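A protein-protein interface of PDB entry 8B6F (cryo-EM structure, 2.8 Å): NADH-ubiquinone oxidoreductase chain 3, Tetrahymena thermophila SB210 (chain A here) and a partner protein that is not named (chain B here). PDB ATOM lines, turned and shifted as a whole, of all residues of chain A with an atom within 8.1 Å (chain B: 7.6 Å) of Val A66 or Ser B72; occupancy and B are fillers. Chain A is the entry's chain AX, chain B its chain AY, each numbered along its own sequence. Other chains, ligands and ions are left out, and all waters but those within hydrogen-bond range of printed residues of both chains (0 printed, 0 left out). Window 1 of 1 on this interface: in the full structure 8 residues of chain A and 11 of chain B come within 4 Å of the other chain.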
ATOM      1  N   PHE A  59      -6.601   6.773 -21.534  1.00  0.00           N
ATOM      2  CA  PHE A  59      -6.994   6.197 -20.252  1.00  0.00           C
ATOM      3  C   PHE A  59      -7.422   7.322 -19.311  1.00  0.00           C
ATOM      4  O   PHE A  59      -6.780   7.621 -18.305  1.00  0.00           O
ATOM      5  CB  PHE A  59      -5.838   5.381 -19.677  1.00  0.00           C
ATOM      6  CG  PHE A  59      -6.208   4.504 -18.509  1.00  0.00           C
ATOM      7  CD1 PHE A  59      -7.530   4.285 -18.156  1.00  0.00           C
ATOM      8  CD2 PHE A  59      -5.212   3.900 -17.761  1.00  0.00           C
ATOM      9  CE1 PHE A  59      -7.846   3.477 -17.081  1.00  0.00           C
ATOM     10  CE2 PHE A  59      -5.523   3.091 -16.688  1.00  0.00           C
ATOM     11  CZ  PHE A  59      -6.840   2.879 -16.347  1.00  0.00           C
ATOM     12  N   PHE A  61     -10.150   7.385 -17.546  1.00  0.00           N
ATOM     13  CA  PHE A  61     -10.944   6.882 -16.430  1.00  0.00           C
ATOM     14  C   PHE A  61     -10.069   6.120 -15.439  1.00  0.00           C
ATOM     15  O   PHE A  61     -10.536   5.203 -14.763  1.00  0.00           O
ATOM     16  CB  PHE A  61     -12.082   5.996 -16.933  1.00  0.00           C
ATOM     17  CG  PHE A  61     -11.622   4.798 -17.712  1.00  0.00           C
ATOM     18  CD1 PHE A  61     -11.409   4.887 -19.077  1.00  0.00           C
ATOM     19  CD2 PHE A  61     -11.412   3.582 -17.084  1.00  0.00           C
ATOM     20  CE1 PHE A  61     -10.988   3.788 -19.800  1.00  0.00           C
ATOM     21  CE2 PHE A  61     -10.993   2.480 -17.802  1.00  0.00           C
ATOM     22  CZ  PHE A  61     -10.780   2.583 -19.161  1.00  0.00           C
ATOM     23  N   PHE A  62      -8.794   6.502 -15.338  1.00  0.00           N
ATOM     24  CA  PHE A  62      -7.854   5.772 -14.497  1.00  0.00           C
ATOM     25  C   PHE A  62      -8.148   5.921 -13.012  1.00  0.00           C
ATOM     26  O   PHE A  62      -7.708   5.080 -12.222  1.00  0.00           O
ATOM     27  CB  PHE A  62      -6.423   6.231 -14.782  1.00  0.00           C
ATOM     28  CG  PHE A  62      -6.168   7.676 -14.457  1.00  0.00           C
ATOM     29  CD1 PHE A  62      -5.718   8.045 -13.201  1.00  0.00           C
ATOM     30  CD2 PHE A  62      -6.349   8.659 -15.413  1.00  0.00           C
ATOM     31  CE1 PHE A  62      -5.472   9.368 -12.899  1.00  0.00           C
ATOM     32  CE2 PHE A  62      -6.103   9.985 -15.119  1.00  0.00           C
ATOM     33  CZ  PHE A  62      -5.664  10.340 -13.860  1.00  0.00           C
ATOM     34  N   MET A  63      -8.879   6.961 -12.607  1.00  0.00           N
ATOM     35  CA  MET A  63      -9.219   7.105 -11.196  1.00  0.00           C
ATOM     36  C   MET A  63     -10.082   5.951 -10.714  1.00  0.00           C
ATOM     37  O   MET A  63      -9.986   5.547  -9.549  1.00  0.00           O
ATOM     38  CB  MET A  63      -9.938   8.432 -10.960  1.00  0.00           C
ATOM     39  CG  MET A  63      -9.080   9.658 -11.218  1.00  0.00           C
ATOM     40  SD  MET A  63      -7.552   9.679 -10.260  1.00  0.00           S
ATOM     41  CE  MET A  63      -8.177   9.526  -8.590  1.00  0.00           C
ATOM     42  N   LEU A  64     -10.926   5.408 -11.588  1.00  0.00           N
ATOM     43  CA  LEU A  64     -11.751   4.271 -11.204  1.00  0.00           C
ATOM     44  C   LEU A  64     -10.893   3.060 -10.866  1.00  0.00           C
ATOM     45  O   LEU A  64     -11.149   2.366  -9.875  1.00  0.00           O
ATOM     46  CB  LEU A  64     -12.724   3.949 -12.330  1.00  0.00           C
ATOM     47  CG  LEU A  64     -13.702   5.083 -12.631  1.00  0.00           C
ATOM     48  CD1 LEU A  64     -14.408   4.756 -13.903  1.00  0.00           C
ATOM     49  CD2 LEU A  64     -14.696   5.287 -11.499  1.00  0.00           C
ATOM     50  N   ALA A  65      -9.875   2.783 -11.680  1.00  0.00           N
ATOM     51  CA  ALA A  65      -8.967   1.688 -11.360  1.00  0.00           C
ATOM     52  C   ALA A  65      -8.168   1.998 -10.101  1.00  0.00           C
ATOM     53  O   ALA A  65      -7.937   1.111  -9.272  1.00  0.00           O
ATOM     54  CB  ALA A  65      -8.033   1.417 -12.538  1.00  0.00           C
ATOM     55  N   VAL A  66      -7.737   3.251  -9.945  1.00  0.00           N
ATOM     56  CA  VAL A  66      -6.993   3.640  -8.750  1.00  0.00           C
ATOM     57  C   VAL A  66      -7.815   3.355  -7.502  1.00  0.00           C
ATOM     58  O   VAL A  66      -7.305   2.817  -6.512  1.00  0.00           O
ATOM     59  CB  VAL A  66      -6.593   5.125  -8.839  1.00  0.00           C
ATOM     60  CG1 VAL A  66      -6.205   5.675  -7.472  1.00  0.00           C
ATOM     61  CG2 VAL A  66      -5.455   5.305  -9.826  1.00  0.00           C
ATOM     62  N   PHE A  67      -9.098   3.712  -7.528  1.00  0.00           N
ATOM     63  CA  PHE A  67      -9.957   3.493  -6.373  1.00  0.00           C
ATOM     64  C   PHE A  67     -10.335   2.029  -6.222  1.00  0.00           C
ATOM     65  O   PHE A  67     -10.553   1.560  -5.100  1.00  0.00           O
ATOM     66  CB  PHE A  67     -11.209   4.362  -6.484  1.00  0.00           C
ATOM     67  CG  PHE A  67     -10.930   5.836  -6.415  1.00  0.00           C
ATOM     68  CD1 PHE A  67     -10.001   6.342  -5.521  1.00  0.00           C
ATOM     69  CD2 PHE A  67     -11.591   6.715  -7.253  1.00  0.00           C
ATOM     70  CE1 PHE A  67      -9.742   7.694  -5.460  1.00  0.00           C
ATOM     71  CE2 PHE A  67     -11.337   8.065  -7.197  1.00  0.00           C
ATOM     72  CZ  PHE A  67     -10.411   8.558  -6.299  1.00  0.00           C
ATOM     73  N   LEU A  68     -10.417   1.292  -7.329  1.00  0.00           N
ATOM     74  CA  LEU A  68     -10.682  -0.139  -7.231  1.00  0.00           C
ATOM     75  C   LEU A  68      -9.560  -0.850  -6.491  1.00  0.00           C
ATOM     76  O   LEU A  68      -9.811  -1.765  -5.698  1.00  0.00           O
ATOM     77  CB  LEU A  68     -10.863  -0.736  -8.625  1.00  0.00           C
ATOM     78  CG  LEU A  68     -11.136  -2.242  -8.651  1.00  0.00           C
ATOM     79  CD1 LEU A  68     -12.496  -2.543  -8.054  1.00  0.00           C
ATOM     80  CD2 LEU A  68     -11.046  -2.778 -10.061  1.00  0.00           C
ATOM     81  N   ILE A  69      -8.313  -0.455  -6.744  1.00  0.00           N
ATOM     82  CA  ILE A  69      -7.185  -1.085  -6.065  1.00  0.00           C
ATOM     83  C   ILE A  69      -7.341  -0.966  -4.555  1.00  0.00           C
ATOM     84  O   ILE A  69      -7.093  -1.923  -3.812  1.00  0.00           O
ATOM     85  CB  ILE A  69      -5.860  -0.468  -6.551  1.00  0.00           C
ATOM     86  CG1 ILE A  69      -5.631  -0.800  -8.027  1.00  0.00           C
ATOM     87  CG2 ILE A  69      -4.691  -0.970  -5.714  1.00  0.00           C
ATOM     88  CD1 ILE A  69      -4.539   0.023  -8.677  1.00  0.00           C
ATOM     89  N   LEU A  70      -7.755   0.209  -4.075  1.00  0.00           N
ATOM     90  CA  LEU A  70      -7.917   0.400  -2.637  1.00  0.00           C
ATOM     91  C   LEU A  70      -9.145  -0.330  -2.108  1.00  0.00           C
ATOM     92  O   LEU A  70      -9.083  -0.978  -1.058  1.00  0.00           O
ATOM     93  CB  LEU A  70      -8.011   1.892  -2.318  1.00  0.00           C
ATOM     94  CG  LEU A  70      -6.893   2.779  -2.868  1.00  0.00           C
ATOM     95  CD1 LEU A  70      -7.130   4.231  -2.490  1.00  0.00           C
ATOM     96  CD2 LEU A  70      -5.536   2.314  -2.370  1.00  0.00           C
ATOM     97  N   TYR A  71     -10.272  -0.232  -2.816  1.00  0.00           N
ATOM     98  CA  TYR A  71     -11.520  -0.767  -2.282  1.00  0.00           C
ATOM     99  C   TYR A  71     -11.550  -2.288  -2.315  1.00  0.00           C
ATOM    100  O   TYR A  71     -12.261  -2.904  -1.513  1.00  0.00           O
ATOM    101  CB  TYR A  71     -12.706  -0.185  -3.049  1.00  0.00           C
ATOM    102  CG  TYR A  71     -12.806   1.321  -2.942  1.00  0.00           C
ATOM    103  CD1 TYR A  71     -12.264   2.003  -1.858  1.00  0.00           C
ATOM    104  CD2 TYR A  71     -13.433   2.064  -3.928  1.00  0.00           C
ATOM    105  CE1 TYR A  71     -12.350   3.375  -1.758  1.00  0.00           C
ATOM    106  CE2 TYR A  71     -13.523   3.439  -3.837  1.00  0.00           C
ATOM    107  CZ  TYR A  71     -12.979   4.087  -2.750  1.00  0.00           C
ATOM    108  OH  TYR A  71     -13.065   5.456  -2.656  1.00  0.00           O
ATOM    109  N   ASP A  72     -10.799  -2.916  -3.220  1.00  0.00           N
ATOM    110  CA  ASP A  72     -10.688  -4.370  -3.186  1.00  0.00           C
ATOM    111  C   ASP A  72     -10.073  -4.830  -1.873  1.00  0.00           C
ATOM    112  O   ASP A  72     -10.557  -5.776  -1.242  1.00  0.00           O
ATOM    113  CB  ASP A  72      -9.858  -4.869  -4.368  1.00  0.00           C
ATOM    114  CG  ASP A  72     -10.653  -4.930  -5.655  1.00  0.00           C
ATOM    115  OD1 ASP A  72     -11.863  -4.620  -5.623  1.00  0.00           O
ATOM    116  OD2 ASP A  72     -10.072  -5.296  -6.699  1.00  0.00           O
ATOM    117  N   ASP A 110     -14.773  11.022  -2.760  1.00  0.00           N
ATOM    118  CA  ASP A 110     -14.578  10.854  -4.195  1.00  0.00           C
ATOM    119  C   ASP A 110     -15.735  11.467  -4.974  1.00  0.00           C
ATOM    120  O   ASP A 110     -15.521  12.165  -5.972  1.00  0.00           O
ATOM    121  CB  ASP A 110     -14.430   9.371  -4.533  1.00  0.00           C
ATOM    122  CG  ASP A 110     -13.245   8.731  -3.836  1.00  0.00           C
ATOM    123  OD1 ASP A 110     -12.255   9.444  -3.571  1.00  0.00           O
ATOM    124  OD2 ASP A 110     -13.300   7.517  -3.553  1.00  0.00           O
ATOM    125  N   LEU B  30       7.730  -0.276 -10.873  1.00  0.00           N
ATOM    126  CA  LEU B  30       6.492  -0.492 -10.134  1.00  0.00           C
ATOM    127  C   LEU B  30       6.140  -1.973 -10.073  1.00  0.00           C
ATOM    128  O   LEU B  30       5.733  -2.476  -9.020  1.00  0.00           O
ATOM    129  CB  LEU B  30       5.360   0.306 -10.781  1.00  0.00           C
ATOM    130  CG  LEU B  30       4.042   0.411 -10.010  1.00  0.00           C
ATOM    131  CD1 LEU B  30       4.231   1.157  -8.700  1.00  0.00           C
ATOM    132  CD2 LEU B  30       2.985   1.087 -10.865  1.00  0.00           C
ATOM    133  N   GLU B  34       5.921  -4.343  -6.684  1.00  0.00           N
ATOM    134  CA  GLU B  34       4.811  -5.233  -6.360  1.00  0.00           C
ATOM    135  C   GLU B  34       5.309  -6.647  -6.094  1.00  0.00           C
ATOM    136  O   GLU B  34       4.854  -7.306  -5.152  1.00  0.00           O
ATOM    137  CB  GLU B  34       3.790  -5.229  -7.498  1.00  0.00           C
ATOM    138  CG  GLU B  34       2.548  -6.060  -7.221  1.00  0.00           C
ATOM    139  CD  GLU B  34       1.773  -5.567  -6.016  1.00  0.00           C
ATOM    140  OE1 GLU B  34       1.974  -4.403  -5.613  1.00  0.00           O
ATOM    141  OE2 GLU B  34       0.965  -6.346  -5.468  1.00  0.00           O
ATOM    142  N   GLY B  65      -2.605  -4.509   1.498  1.00  0.00           N
ATOM    143  CA  GLY B  65      -3.137  -3.156   1.463  1.00  0.00           C
ATOM    144  C   GLY B  65      -2.079  -2.108   1.193  1.00  0.00           C
ATOM    145  O   GLY B  65      -2.298  -1.181   0.411  1.00  0.00           O
ATOM    146  N   VAL B  66      -0.922  -2.229   1.842  1.00  0.00           N
ATOM    147  CA  VAL B  66       0.152  -1.273   1.599  1.00  0.00           C
ATOM    148  C   VAL B  66       0.607  -1.360   0.149  1.00  0.00           C
ATOM    149  O   VAL B  66       0.865  -0.340  -0.501  1.00  0.00           O
ATOM    150  CB  VAL B  66       1.311  -1.507   2.584  1.00  0.00           C
ATOM    151  CG1 VAL B  66       2.497  -0.615   2.249  1.00  0.00           C
ATOM    152  CG2 VAL B  66       0.844  -1.258   4.008  1.00  0.00           C
ATOM    153  N   ALA B  67       0.721  -2.581  -0.378  1.00  0.00           N
ATOM    154  CA  ALA B  67       1.107  -2.744  -1.774  1.00  0.00           C
ATOM    155  C   ALA B  67       0.075  -2.130  -2.708  1.00  0.00           C
ATOM    156  O   ALA B  67       0.431  -1.492  -3.704  1.00  0.00           O
ATOM    157  CB  ALA B  67       1.298  -4.227  -2.095  1.00  0.00           C
ATOM    158  N   GLY B  68      -1.211  -2.310  -2.404  1.00  0.00           N
ATOM    159  CA  GLY B  68      -2.241  -1.707  -3.234  1.00  0.00           C
ATOM    160  C   GLY B  68      -2.175  -0.193  -3.237  1.00  0.00           C
ATOM    161  O   GLY B  68      -2.287   0.440  -4.289  1.00  0.00           O
ATOM    162  N   LEU B  69      -1.992   0.410  -2.061  1.00  0.00           N
ATOM    163  CA  LEU B  69      -1.889   1.864  -1.992  1.00  0.00           C
ATOM    164  C   LEU B  69      -0.671   2.365  -2.756  1.00  0.00           C
ATOM    165  O   LEU B  69      -0.753   3.358  -3.488  1.00  0.00           O
ATOM    166  CB  LEU B  69      -1.835   2.317  -0.535  1.00  0.00           C
ATOM    167  CG  LEU B  69      -1.731   3.828  -0.309  1.00  0.00           C
ATOM    168  CD1 LEU B  69      -2.920   4.561  -0.913  1.00  0.00           C
ATOM    169  CD2 LEU B  69      -1.614   4.130   1.172  1.00  0.00           C
ATOM    170  N   GLU B  70       0.470   1.693  -2.595  1.00  0.00           N
ATOM    171  CA  GLU B  70       1.673   2.103  -3.311  1.00  0.00           C
ATOM    172  C   GLU B  70       1.496   1.939  -4.814  1.00  0.00           C
ATOM    173  O   GLU B  70       1.990   2.755  -5.599  1.00  0.00           O
ATOM    174  CB  GLU B  70       2.882   1.309  -2.819  1.00  0.00           C
ATOM    175  CG  GLU B  70       3.328   1.694  -1.419  1.00  0.00           C
ATOM    176  CD  GLU B  70       4.681   1.114  -1.057  1.00  0.00           C
ATOM    177  OE1 GLU B  70       5.287   0.435  -1.913  1.00  0.00           O
ATOM    178  OE2 GLU B  70       5.141   1.338   0.082  1.00  0.00           O
ATOM    179  N   PHE B  71       0.790   0.888  -5.234  1.00  0.00           N
ATOM    180  CA  PHE B  71       0.539   0.692  -6.657  1.00  0.00           C
ATOM    181  C   PHE B  71      -0.359   1.791  -7.207  1.00  0.00           C
ATOM    182  O   PHE B  71      -0.155   2.262  -8.331  1.00  0.00           O
ATOM    183  CB  PHE B  71      -0.081  -0.684  -6.898  1.00  0.00           C
ATOM    184  CG  PHE B  71       0.142  -1.211  -8.288  1.00  0.00           C
ATOM    185  CD1 PHE B  71       1.307  -1.892  -8.603  1.00  0.00           C
ATOM    186  CD2 PHE B  71      -0.812  -1.032  -9.276  1.00  0.00           C
ATOM    187  CE1 PHE B  71       1.519  -2.381  -9.878  1.00  0.00           C
ATOM    188  CE2 PHE B  71      -0.606  -1.518 -10.553  1.00  0.00           C
ATOM    189  CZ  PHE B  71       0.560  -2.194 -10.854  1.00  0.00           C
ATOM    190  N   SER B  72      -1.356   2.216  -6.431  1.00  0.00           N
ATOM    191  CA  SER B  72      -2.191   3.335  -6.853  1.00  0.00           C
ATOM    192  C   SER B  72      -1.359   4.597  -7.030  1.00  0.00           C
ATOM    193  O   SER B  72      -1.503   5.317  -8.022  1.00  0.00           O
ATOM    194  CB  SER B  72      -3.300   3.568  -5.828  1.00  0.00           C
ATOM    195  OG  SER B  72      -4.148   2.438  -5.722  1.00  0.00           O
ATOM    196  N   PHE B  73      -0.485   4.888  -6.063  1.00  0.00           N
ATOM    197  CA  PHE B  73       0.383   6.054  -6.181  1.00  0.00           C
ATOM    198  C   PHE B  73       1.293   5.936  -7.394  1.00  0.00           C
ATOM    199  O   PHE B  73       1.530   6.923  -8.102  1.00  0.00           O
ATOM    200  CB  PHE B  73       1.207   6.228  -4.906  1.00  0.00           C
ATOM    201  CG  PHE B  73       0.432   6.799  -3.752  1.00  0.00           C
ATOM    202  CD1 PHE B  73      -0.401   7.892  -3.928  1.00  0.00           C
ATOM    203  CD2 PHE B  73       0.539   6.243  -2.491  1.00  0.00           C
ATOM    204  CE1 PHE B  73      -1.110   8.418  -2.870  1.00  0.00           C
ATOM    205  CE2 PHE B  73      -0.170   6.765  -1.426  1.00  0.00           C
ATOM    206  CZ  PHE B  73      -0.996   7.854  -1.617  1.00  0.00           C
ATOM    207  N   GLY B  74       1.809   4.736  -7.653  1.00  0.00           N
ATOM    208  CA  GLY B  74       2.665   4.543  -8.811  1.00  0.00           C
ATOM    209  C   GLY B  74       1.938   4.768 -10.121  1.00  0.00           C
ATOM    210  O   GLY B  74       2.483   5.369 -11.049  1.00  0.00           O
ATOM    211  N   ILE B  75       0.698   4.290 -10.219  1.00  0.00           N
ATOM    212  CA  ILE B  75      -0.095   4.545 -11.417  1.00  0.00           C
ATOM    213  C   ILE B  75      -0.269   6.043 -11.622  1.00  0.00           C
ATOM    214  O   ILE B  75      -0.121   6.559 -12.736  1.00  0.00           O
ATOM    215  CB  ILE B  75      -1.454   3.830 -11.320  1.00  0.00           C
ATOM    216  CG1 ILE B  75      -1.263   2.316 -11.411  1.00  0.00           C
ATOM    217  CG2 ILE B  75      -2.408   4.322 -12.411  1.00  0.00           C
ATOM    218  CD1 ILE B  75      -2.518   1.521 -11.127  1.00  0.00           C
ATOM    219  N   LEU B  76      -0.594   6.763 -10.549  1.00  0.00           N
ATOM    220  CA  LEU B  76      -0.803   8.200 -10.666  1.00  0.00           C
ATOM    221  C   LEU B  76       0.469   8.910 -11.113  1.00  0.00           C
ATOM    222  O   LEU B  76       0.420   9.810 -11.958  1.00  0.00           O
ATOM    223  CB  LEU B  76      -1.299   8.762  -9.338  1.00  0.00           C
ATOM    224  CG  LEU B  76      -2.715   8.347  -8.928  1.00  0.00           C
ATOM    225  CD1 LEU B  76      -3.048   8.881  -7.552  1.00  0.00           C
ATOM    226  CD2 LEU B  76      -3.745   8.826  -9.936  1.00  0.00           C
ATOM    227  N   ILE B  77       1.617   8.526 -10.554  1.00  0.00           N
ATOM    228  CA  ILE B  77       2.870   9.166 -10.941  1.00  0.00           C
ATOM    229  C   ILE B  77       3.206   8.845 -12.392  1.00  0.00           C
ATOM    230  O   ILE B  77       3.660   9.715 -13.144  1.00  0.00           O
ATOM    231  CB  ILE B  77       4.006   8.749  -9.989  1.00  0.00           C
ATOM    232  CG1 ILE B  77       3.702   9.213  -8.563  1.00  0.00           C
ATOM    233  CG2 ILE B  77       5.338   9.337 -10.451  1.00  0.00           C
ATOM    234  CD1 ILE B  77       4.624   8.625  -7.515  1.00  0.00           C
ATOM    235  N   ALA B  78       2.997   7.595 -12.809  1.00  0.00           N
ATOM    236  CA  ALA B  78       3.277   7.226 -14.193  1.00  0.00           C
ATOM    237  C   ALA B  78       2.414   8.021 -15.165  1.00  0.00           C
ATOM    238  O   ALA B  78       2.866   8.382 -16.256  1.00  0.00           O
ATOM    239  CB  ALA B  78       3.058   5.727 -14.389  1.00  0.00           C
ATOM    240  N   ILE B  79       1.162   8.286 -14.794  1.00  0.00           N
ATOM    241  CA  ILE B  79       0.298   9.107 -15.636  1.00  0.00           C
ATOM    242  C   ILE B  79       0.756  10.557 -15.606  1.00  0.00           C
ATOM    243  O   ILE B  79       0.738  11.252 -16.628  1.00  0.00           O
ATOM    244  CB  ILE B  79      -1.171   8.953 -15.206  1.00  0.00           C
ATOM    245  CG1 ILE B  79      -1.659   7.548 -15.568  1.00  0.00           C
ATOM    246  CG2 ILE B  79      -2.045  10.024 -15.861  1.00  0.00           C
ATOM    247  CD1 ILE B  79      -3.034   7.221 -15.063  1.00  0.00           C
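Among the printed residues, merely in contact across the chains: Phe A62 with Leu B76 (3.5 Å), Phe A62 with Ile B79 (3.2 Å), Met A63 with Leu B76 (3.9 Å), Val A66 with Leu B76 (3.9 Å), Ile A69 with Gly B68 (3.1 Å), Ile A69 with Phe B71 (3.9 Å), Ile A69 with Ser B72 (3.5 Å), Ile A69 with Ile B75 (3.5 Å), Leu A70 with Leu B69 (3.7 Å) and Leu A70 with Ser B72 (3.6 Å).
O of Gly B68 lies within hydrogen-bond range of OG of Ser B72 (3.1 Å).
Phe A61 touches none of the printed residues of chain B.
No residue of chain B comes within 4 Å of Ala A65.
Of chain B, only Ser B72 (3.3 Å) and Leu B76 (3.9 Å) come within 4 Å of Val A66.
Of the printed residues of chain B, Ile A69 touches Gly B68 (3.1 Å), Phe B71 (3.9 Å), Ser B72 (3.5 Å) and Ile B75 (3.5 Å).
Val B66 touches none of the printed residues of chain A.
Printed residues of chain A within 4 Å of Gly B68: Ile A69.
Of the printed residues of chain A, Phe B71 touches Ile A69 (3.9 Å).
The nearest residue of chain B that does not touch Val A66 is Ile B75 (4.1 Å).
The nearest printed residue of chain A that does not touch Ile B79 is Phe A59 (4.8 Å).
Of the 14 printed residues of chain A, 5 touch a printed residue of chain B.
Printed residues of chain A that touch a printed residue of chain B: Phe A62, Met A63, Val A66, Ile A69 and Leu A70.
Hydrophobic or aromatic side chains of chain A within 4 Å of the printed part of chain B: Phe A62, Met A63, Val A66, Ile A69 and Leu A70.
Hydrophobic or aromatic side chains of chain B within 4 Å of the printed part of chain A: Leu B69, Phe B71, Ile B75, Leu B76 and Ile B79.
Among the printed residues, 11 pairs touch across the chains.
Among the printed residues, no Asp or Glu carboxylate lies within 4 Å of a Lys or Arg side-chain nitrogen of the other chain.
The backbone carbonyl oxygen (O) of Val A66 lies within hydrogen-bond range of the side-chain hydroxyl (OG) of Ser B72.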
